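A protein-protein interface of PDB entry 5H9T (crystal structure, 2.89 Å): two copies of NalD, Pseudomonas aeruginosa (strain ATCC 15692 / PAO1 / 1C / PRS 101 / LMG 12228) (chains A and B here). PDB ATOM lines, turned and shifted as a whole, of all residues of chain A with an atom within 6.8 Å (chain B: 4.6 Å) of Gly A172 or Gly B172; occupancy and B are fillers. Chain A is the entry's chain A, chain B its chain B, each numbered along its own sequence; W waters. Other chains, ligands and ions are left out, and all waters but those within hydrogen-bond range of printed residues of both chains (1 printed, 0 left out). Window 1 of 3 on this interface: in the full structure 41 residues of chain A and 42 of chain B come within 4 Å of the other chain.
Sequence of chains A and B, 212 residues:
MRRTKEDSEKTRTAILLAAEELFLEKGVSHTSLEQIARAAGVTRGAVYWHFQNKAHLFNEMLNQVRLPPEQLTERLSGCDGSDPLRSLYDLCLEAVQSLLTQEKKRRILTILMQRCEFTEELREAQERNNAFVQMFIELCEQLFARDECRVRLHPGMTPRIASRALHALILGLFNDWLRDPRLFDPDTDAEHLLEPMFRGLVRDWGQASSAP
A ring nitrogen (ND1) of His A167 is in hydrogen-bond range of the side-chain carboxylate of Asp B176, at 2.7 Å.
The guanidinium group (NH2) of Arg A179 lies within salt-bridge range of the side-chain carboxylate (OD1) of Asp A176 (2.5 Å).
Among the printed residues, pairs that only touch across the chains: Ala A168 with Ala B168 (3.8 Å), Ala A168 with Gly B172 (3.1 Å), Ala A168 with Leu B173 (3.5 Å), Ala A168 with Asp B176 (3.6 Å), Leu A169 with Ala B168 (3.96 Å), Leu A169 with Leu B169 (3.9 Å), Leu A171 with Gly B172 (3.96 Å), Leu A171 with Asn B175 (3.9 Å), Leu A171 with Asp B176 (3.1 Å), Gly A172 with Ala B168 (3.2 Å), Gly A172 with Leu B171 (3.997 Å), Gly A172 with Gly B172 (3.8 Å), Leu A173 with Ala B168 (3.2 Å), Asn A175 with Leu B171 (3.9 Å), Asn A175 with Asn B175 (3.5 Å), Asp A176 with Ala B168 (3.7 Å) and Asp A176 with Leu B171 (3.1 Å).
Printed residues of chain B within 4 Å of Gly A172: Ala B168 (3.2 Å), Leu B171 (3.997 Å) and Gly B172 (3.8 Å).
Gly B172 touches three residues of chain A.
Printed residues of chain A within 4 Å of Ala B168: Ala A168 (3.8 Å), Leu A169 (3.96 Å), Gly A172 (3.2 Å), Leu A173 (3.2 Å) and Asp A176 (3.7 Å).
Of the printed residues of chain B, Asn A175 touches Leu B171 (3.9 Å) and Asn B175 (3.5 Å).
The nearest residue of chain A that does not touch Gly B172 is Leu A169 (5.0 Å).
Hydrophobic or aromatic side chains of chain A within 4 Å of the printed part of chain B: His A167, Ala A168, Leu A169, Leu A171 and Leu A173.
Along chain B the printed residues that touch a printed residue of chain A span positions 168 to 176.
Among the printed residues, no Asp or Glu carboxylate lies within 4 Å of a Lys or Arg side-chain nitrogen of the other chain.
Ala A168 touches its own counterpart, Ala B168.
Ala A168 touches Gly B172, and with the chains exchanged Gly A172 touches Ala B168.
Ala A168 touches Leu B173, and with the chains exchanged Leu A173 touches Ala B168.
Ala A168 touches Asp B176, and with the chains exchanged Asp A176 touches Ala B168.
Positions printed for both chains: 168, 169, 170, 171, 172, 173, 174, 175 and 176.
Water W1 lies within hydrogen-bond range of the backbone carbonyl oxygen of Arg A164 (2.8 Å) and the side-chain carboxylate of Asp B176 (2.8 Å).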
ATOM      1  N   ARG A 164      -3.012  32.548  30.570  1.00  0.00           N
ATOM      2  CA  ARG A 164      -1.970  32.133  29.627  1.00  0.00           C
ATOM      3  C   ARG A 164      -1.113  31.005  30.165  1.00  0.00           C
ATOM      4  O   ARG A 164      -0.753  30.090  29.417  1.00  0.00           O
ATOM      5  CB  ARG A 164      -1.105  33.315  29.234  1.00  0.00           C
ATOM      6  CG  ARG A 164      -1.835  34.208  28.256  1.00  0.00           C
ATOM      7  CD  ARG A 164      -1.370  35.640  28.310  1.00  0.00           C
ATOM      8  NE  ARG A 164      -2.153  36.450  27.372  1.00  0.00           N
ATOM      9  CZ  ARG A 164      -3.406  36.855  27.556  1.00  0.00           C
ATOM     10  NH1 ARG A 164      -4.102  36.529  28.635  1.00  0.00           N
ATOM     11  NH2 ARG A 164      -3.970  37.607  26.638  1.00  0.00           N
ATOM     12  N   HIS A 167      -3.341  27.930  29.930  1.00  0.00           N
ATOM     13  CA  HIS A 167      -3.528  27.430  28.580  1.00  0.00           C
ATOM     14  C   HIS A 167      -2.264  26.739  28.071  1.00  0.00           C
ATOM     15  O   HIS A 167      -2.347  25.657  27.493  1.00  0.00           O
ATOM     16  CB  HIS A 167      -3.934  28.510  27.589  1.00  0.00           C
ATOM     17  CG  HIS A 167      -4.136  27.975  26.213  1.00  0.00           C
ATOM     18  ND1 HIS A 167      -3.197  28.103  25.217  1.00  0.00           N
ATOM     19  CD2 HIS A 167      -5.141  27.236  25.693  1.00  0.00           C
ATOM     20  CE1 HIS A 167      -3.634  27.503  24.125  1.00  0.00           C
ATOM     21  NE2 HIS A 167      -4.813  26.971  24.386  1.00  0.00           N
ATOM     22  N   ALA A 168      -1.110  27.366  28.297  1.00  0.00           N
ATOM     23  CA  ALA A 168       0.159  26.772  27.925  1.00  0.00           C
ATOM     24  C   ALA A 168       0.289  25.375  28.512  1.00  0.00           C
ATOM     25  O   ALA A 168       0.688  24.440  27.822  1.00  0.00           O
ATOM     26  CB  ALA A 168       1.316  27.645  28.382  1.00  0.00           C
ATOM     27  N   LEU A 169      -0.056  25.216  29.780  1.00  0.00           N
ATOM     28  CA  LEU A 169       0.022  23.893  30.401  1.00  0.00           C
ATOM     29  C   LEU A 169      -0.838  22.882  29.676  1.00  0.00           C
ATOM     30  O   LEU A 169      -0.375  21.783  29.364  1.00  0.00           O
ATOM     31  CB  LEU A 169      -0.404  23.935  31.868  1.00  0.00           C
ATOM     32  CG  LEU A 169      -0.372  22.573  32.572  1.00  0.00           C
ATOM     33  CD1 LEU A 169       0.994  21.924  32.434  1.00  0.00           C
ATOM     34  CD2 LEU A 169      -0.734  22.738  34.036  1.00  0.00           C
ATOM     35  N   ILE A 170      -2.094  23.234  29.402  1.00  0.00           N
ATOM     36  CA  ILE A 170      -3.012  22.287  28.747  1.00  0.00           C
ATOM     37  C   ILE A 170      -2.470  21.948  27.375  1.00  0.00           C
ATOM     38  O   ILE A 170      -2.458  20.796  26.967  1.00  0.00           O
ATOM     39  CB  ILE A 170      -4.427  22.834  28.530  1.00  0.00           C
ATOM     40  CG1 ILE A 170      -5.048  23.357  29.817  1.00  0.00           C
ATOM     41  CG2 ILE A 170      -5.312  21.751  27.939  1.00  0.00           C
ATOM     42  CD1 ILE A 170      -5.328  22.301  30.852  1.00  0.00           C
ATOM     43  N   LEU A 171      -2.059  22.978  26.655  1.00  0.00           N
ATOM     44  CA  LEU A 171      -1.507  22.802  25.326  1.00  0.00           C
ATOM     45  C   LEU A 171      -0.297  21.894  25.354  1.00  0.00           C
ATOM     46  O   LEU A 171      -0.169  20.996  24.532  1.00  0.00           O
ATOM     47  CB  LEU A 171      -1.109  24.154  24.746  1.00  0.00           C
ATOM     48  CG  LEU A 171      -0.602  24.099  23.312  1.00  0.00           C
ATOM     49  CD1 LEU A 171      -1.638  23.497  22.383  1.00  0.00           C
ATOM     50  CD2 LEU A 171      -0.204  25.502  22.864  1.00  0.00           C
ATOM     51  N   GLY A 172       0.599  22.160  26.290  1.00  0.00           N
ATOM     52  CA  GLY A 172       1.809  21.371  26.440  1.00  0.00           C
ATOM     53  C   GLY A 172       1.529  19.923  26.779  1.00  0.00           C
ATOM     54  O   GLY A 172       2.221  19.030  26.304  1.00  0.00           O
ATOM     55  N   LEU A 173       0.498  19.671  27.544  1.00  0.00           N
ATOM     56  CA  LEU A 173       0.168  18.321  27.901  1.00  0.00           C
ATOM     57  C   LEU A 173      -0.341  17.588  26.702  1.00  0.00           C
ATOM     58  O   LEU A 173       0.000  16.471  26.459  1.00  0.00           O
ATOM     59  CB  LEU A 173      -0.883  18.306  28.998  1.00  0.00           C
ATOM     60  CG  LEU A 173      -0.399  18.629  30.391  1.00  0.00           C
ATOM     61  CD1 LEU A 173      -1.529  18.551  31.373  1.00  0.00           C
ATOM     62  CD2 LEU A 173       0.751  17.763  30.823  1.00  0.00           C
ATOM     63  N   PHE A 174      -1.189  18.231  25.943  1.00  0.00           N
ATOM     64  CA  PHE A 174      -1.715  17.633  24.722  1.00  0.00           C
ATOM     65  C   PHE A 174      -0.558  17.323  23.795  1.00  0.00           C
ATOM     66  O   PHE A 174      -0.419  16.211  23.285  1.00  0.00           O
ATOM     67  CB  PHE A 174      -2.691  18.588  24.023  1.00  0.00           C
ATOM     68  CG  PHE A 174      -4.108  18.472  24.505  1.00  0.00           C
ATOM     69  CD1 PHE A 174      -4.395  18.515  25.842  1.00  0.00           C
ATOM     70  CD2 PHE A 174      -5.154  18.336  23.602  1.00  0.00           C
ATOM     71  CE1 PHE A 174      -5.700  18.409  26.288  1.00  0.00           C
ATOM     72  CE2 PHE A 174      -6.463  18.230  24.033  1.00  0.00           C
ATOM     73  CZ  PHE A 174      -6.739  18.269  25.383  1.00  0.00           C
ATOM     74  N   ASN A 175       0.287  18.317  23.607  1.00  0.00           N
ATOM     75  CA  ASN A 175       1.405  18.211  22.695  1.00  0.00           C
ATOM     76  C   ASN A 175       2.388  17.112  23.090  1.00  0.00           C
ATOM     77  O   ASN A 175       2.788  16.300  22.257  1.00  0.00           O
ATOM     78  CB  ASN A 175       2.128  19.543  22.617  1.00  0.00           C
ATOM     79  CG  ASN A 175       2.686  19.806  21.251  1.00  0.00           C
ATOM     80  OD1 ASN A 175       3.730  19.272  20.887  1.00  0.00           O
ATOM     81  ND2 ASN A 175       1.993  20.636  20.481  1.00  0.00           N
ATOM     82  N   ASP A 176       2.755  17.080  24.367  1.00  0.00           N
ATOM     83  CA  ASP A 176       3.644  16.043  24.878  1.00  0.00           C
ATOM     84  C   ASP A 176       3.026  14.659  24.703  1.00  0.00           C
ATOM     85  O   ASP A 176       3.672  13.749  24.175  1.00  0.00           O
ATOM     86  CB  ASP A 176       3.974  16.264  26.360  1.00  0.00           C
ATOM     87  CG  ASP A 176       5.310  16.936  26.577  1.00  0.00           C
ATOM     88  OD1 ASP A 176       6.085  17.049  25.614  1.00  0.00           O
ATOM     89  OD2 ASP A 176       5.600  17.336  27.729  1.00  0.00           O
ATOM     90  N   TRP A 177       1.784  14.493  25.147  1.00  0.00           N
ATOM     91  CA  TRP A 177       1.184  13.164  25.150  1.00  0.00           C
ATOM     92  C   TRP A 177       0.978  12.632  23.736  1.00  0.00           C
ATOM     93  O   TRP A 177       1.075  11.424  23.512  1.00  0.00           O
ATOM     94  CB  TRP A 177      -0.146  13.135  25.893  1.00  0.00           C
ATOM     95  CG  TRP A 177      -0.611  11.754  26.105  1.00  0.00           C
ATOM     96  CD1 TRP A 177      -0.247  10.924  27.106  1.00  0.00           C
ATOM     97  CD2 TRP A 177      -1.527  11.019  25.285  1.00  0.00           C
ATOM     98  NE1 TRP A 177      -0.886   9.712  26.971  1.00  0.00           N
ATOM     99  CE2 TRP A 177      -1.675   9.748  25.856  1.00  0.00           C
ATOM    100  CE3 TRP A 177      -2.237  11.315  24.123  1.00  0.00           C
ATOM    101  CZ2 TRP A 177      -2.501   8.773  25.313  1.00  0.00           C
ATOM    102  CZ3 TRP A 177      -3.064  10.335  23.577  1.00  0.00           C
ATOM    103  CH2 TRP A 177      -3.185   9.085  24.172  1.00  0.00           C
ATOM    104  N   LEU A 178       0.671  13.519  22.796  1.00  0.00           N
ATOM    105  CA  LEU A 178       0.433  13.095  21.422  1.00  0.00           C
ATOM    106  C   LEU A 178       1.740  12.767  20.702  1.00  0.00           C
ATOM    107  O   LEU A 178       1.778  11.872  19.884  1.00  0.00           O
ATOM    108  CB  LEU A 178      -0.364  14.145  20.663  1.00  0.00           C
ATOM    109  CG  LEU A 178      -1.823  14.289  21.119  1.00  0.00           C
ATOM    110  CD1 LEU A 178      -2.447  15.520  20.512  1.00  0.00           C
ATOM    111  CD2 LEU A 178      -2.670  13.079  20.782  1.00  0.00           C
ATOM    112  N   ARG A 179       2.821  13.460  21.040  1.00  0.00           N
ATOM    113  CA  ARG A 179       4.153  13.105  20.540  1.00  0.00           C
ATOM    114  C   ARG A 179       4.612  11.773  21.119  1.00  0.00           C
ATOM    115  O   ARG A 179       5.309  11.023  20.457  1.00  0.00           O
ATOM    116  CB  ARG A 179       5.148  14.205  20.918  1.00  0.00           C
ATOM    117  CG  ARG A 179       6.472  14.186  20.159  1.00  0.00           C
ATOM    118  CD  ARG A 179       7.593  15.031  20.788  1.00  0.00           C
ATOM    119  NE  ARG A 179       7.282  15.428  22.159  1.00  0.00           N
ATOM    120  CZ  ARG A 179       7.649  14.757  23.249  1.00  0.00           C
ATOM    121  NH1 ARG A 179       8.367  13.630  23.173  1.00  0.00           N
ATOM    122  NH2 ARG A 179       7.286  15.219  24.438  1.00  0.00           N
ATOM    123  N   PHE A 184       2.571   9.756  30.103  1.00  0.00           N
ATOM    124  CA  PHE A 184       1.623   9.646  31.188  1.00  0.00           C
ATOM    125  C   PHE A 184       0.302   9.030  30.762  1.00  0.00           C
ATOM    126  O   PHE A 184       0.060   8.802  29.578  1.00  0.00           O
ATOM    127  CB  PHE A 184       1.398  11.014  31.859  1.00  0.00           C
ATOM    128  CG  PHE A 184       0.870  12.078  30.949  1.00  0.00           C
ATOM    129  CD1 PHE A 184      -0.507  12.238  30.754  1.00  0.00           C
ATOM    130  CD2 PHE A 184       1.727  12.957  30.331  1.00  0.00           C
ATOM    131  CE1 PHE A 184      -1.015  13.240  29.928  1.00  0.00           C
ATOM    132  CE2 PHE A 184       1.226  13.954  29.497  1.00  0.00           C
ATOM    133  CZ  PHE A 184      -0.149  14.094  29.298  1.00  0.00           C
ATOM    134  N   ALA B 168       5.617  20.065  30.209  1.00  0.00           N
ATOM    135  CA  ALA B 168       4.420  20.427  29.440  1.00  0.00           C
ATOM    136  C   ALA B 168       4.228  21.920  29.482  1.00  0.00           C
ATOM    137  O   ALA B 168       3.979  22.549  28.444  1.00  0.00           O
ATOM    138  CB  ALA B 168       3.189  19.720  29.981  1.00  0.00           C
ATOM    139  N   LEU B 169       4.399  22.511  30.656  1.00  0.00           N
ATOM    140  CA  LEU B 169       4.286  23.971  30.764  1.00  0.00           C
ATOM    141  C   LEU B 169       5.266  24.717  29.859  1.00  0.00           C
ATOM    142  O   LEU B 169       4.864  25.600  29.110  1.00  0.00           O
ATOM    143  CB  LEU B 169       4.474  24.452  32.204  1.00  0.00           C
ATOM    144  CG  LEU B 169       4.360  25.974  32.372  1.00  0.00           C
ATOM    145  CD1 LEU B 169       3.052  26.499  31.807  1.00  0.00           C
ATOM    146  CD2 LEU B 169       4.489  26.346  33.834  1.00  0.00           C
ATOM    147  N   ILE B 170       6.532  24.336  29.905  1.00  0.00           N
ATOM    148  CA  ILE B 170       7.545  25.018  29.108  1.00  0.00           C
ATOM    149  C   ILE B 170       7.223  24.832  27.635  1.00  0.00           C
ATOM    150  O   ILE B 170       7.294  25.776  26.858  1.00  0.00           O
ATOM    151  CB  ILE B 170       8.966  24.466  29.299  1.00  0.00           C
ATOM    152  CG1 ILE B 170       9.377  24.434  30.770  1.00  0.00           C
ATOM    153  CG2 ILE B 170       9.952  25.304  28.507  1.00  0.00           C
ATOM    154  CD1 ILE B 170       9.520  25.792  31.410  1.00  0.00           C
ATOM    155  N   LEU B 171       6.909  23.599  27.259  1.00  0.00           N
ATOM    156  CA  LEU B 171       6.567  23.293  25.896  1.00  0.00           C
ATOM    157  C   LEU B 171       5.371  24.105  25.419  1.00  0.00           C
ATOM    158  O   LEU B 171       5.396  24.676  24.323  1.00  0.00           O
ATOM    159  CB  LEU B 171       6.230  21.816  25.760  1.00  0.00           C
ATOM    160  CG  LEU B 171       5.941  21.355  24.322  1.00  0.00           C
ATOM    161  CD1 LEU B 171       7.129  21.637  23.409  1.00  0.00           C
ATOM    162  CD2 LEU B 171       5.590  19.874  24.326  1.00  0.00           C
ATOM    163  N   GLY B 172       4.333  24.150  26.248  1.00  0.00           N
ATOM    164  CA  GLY B 172       3.135  24.913  25.942  1.00  0.00           C
ATOM    165  C   GLY B 172       3.387  26.402  25.793  1.00  0.00           C
ATOM    166  O   GLY B 172       2.805  27.052  24.923  1.00  0.00           O
ATOM    167  N   LEU B 173       4.274  26.936  26.616  1.00  0.00           N
ATOM    168  CA  LEU B 173       4.616  28.335  26.538  1.00  0.00           C
ATOM    169  C   LEU B 173       5.324  28.656  25.232  1.00  0.00           C
ATOM    170  O   LEU B 173       5.056  29.681  24.599  1.00  0.00           O
ATOM    171  CB  LEU B 173       5.510  28.722  27.712  1.00  0.00           C
ATOM    172  CG  LEU B 173       4.784  28.897  29.052  1.00  0.00           C
ATOM    173  CD1 LEU B 173       5.814  29.064  30.151  1.00  0.00           C
ATOM    174  CD2 LEU B 173       3.836  30.084  29.007  1.00  0.00           C
ATOM    175  N   PHE B 174       6.259  27.799  24.853  1.00  0.00           N
ATOM    176  CA  PHE B 174       6.969  27.957  23.589  1.00  0.00           C
ATOM    177  C   PHE B 174       5.965  27.896  22.443  1.00  0.00           C
ATOM    178  O   PHE B 174       5.939  28.760  21.560  1.00  0.00           O
ATOM    179  CB  PHE B 174       8.023  26.851  23.413  1.00  0.00           C
ATOM    180  CG  PHE B 174       9.346  27.168  24.045  1.00  0.00           C
ATOM    181  CD1 PHE B 174       9.416  27.608  25.340  1.00  0.00           C
ATOM    182  CD2 PHE B 174      10.512  27.034  23.331  1.00  0.00           C
ATOM    183  CE1 PHE B 174      10.631  27.903  25.914  1.00  0.00           C
ATOM    184  CE2 PHE B 174      11.733  27.335  23.898  1.00  0.00           C
ATOM    185  CZ  PHE B 174      11.792  27.772  25.195  1.00  0.00           C
ATOM    186  N   ASN B 175       5.132  26.870  22.487  1.00  0.00           N
ATOM    187  CA  ASN B 175       4.185  26.617  21.425  1.00  0.00           C
ATOM    188  C   ASN B 175       3.181  27.747  21.260  1.00  0.00           C
ATOM    189  O   ASN B 175       2.944  28.211  20.148  1.00  0.00           O
ATOM    190  CB  ASN B 175       3.463  25.311  21.693  1.00  0.00           C
ATOM    191  CG  ASN B 175       3.124  24.582  20.430  1.00  0.00           C
ATOM    192  OD1 ASN B 175       2.159  24.923  19.753  1.00  0.00           O
ATOM    193  ND2 ASN B 175       3.921  23.573  20.095  1.00  0.00           N
ATOM    194  N   ASP B 176       2.620  28.206  22.378  1.00  0.00           N
ATOM    195  CA  ASP B 176       1.693  29.336  22.363  1.00  0.00           C
ATOM    196  C   ASP B 176       2.357  30.595  21.813  1.00  0.00           C
ATOM    197  O   ASP B 176       1.827  31.237  20.904  1.00  0.00           O
ATOM    198  CB  ASP B 176       1.133  29.628  23.754  1.00  0.00           C
ATOM    199  CG  ASP B 176      -0.236  29.030  23.980  1.00  0.00           C
ATOM    200  OD1 ASP B 176      -0.861  28.568  23.014  1.00  0.00           O
ATOM    201  OD2 ASP B 176      -0.712  29.034  25.138  1.00  0.00           O
HETATM  202  O   HOH W   1      -0.056  31.126  26.914  1.00  0.00           O
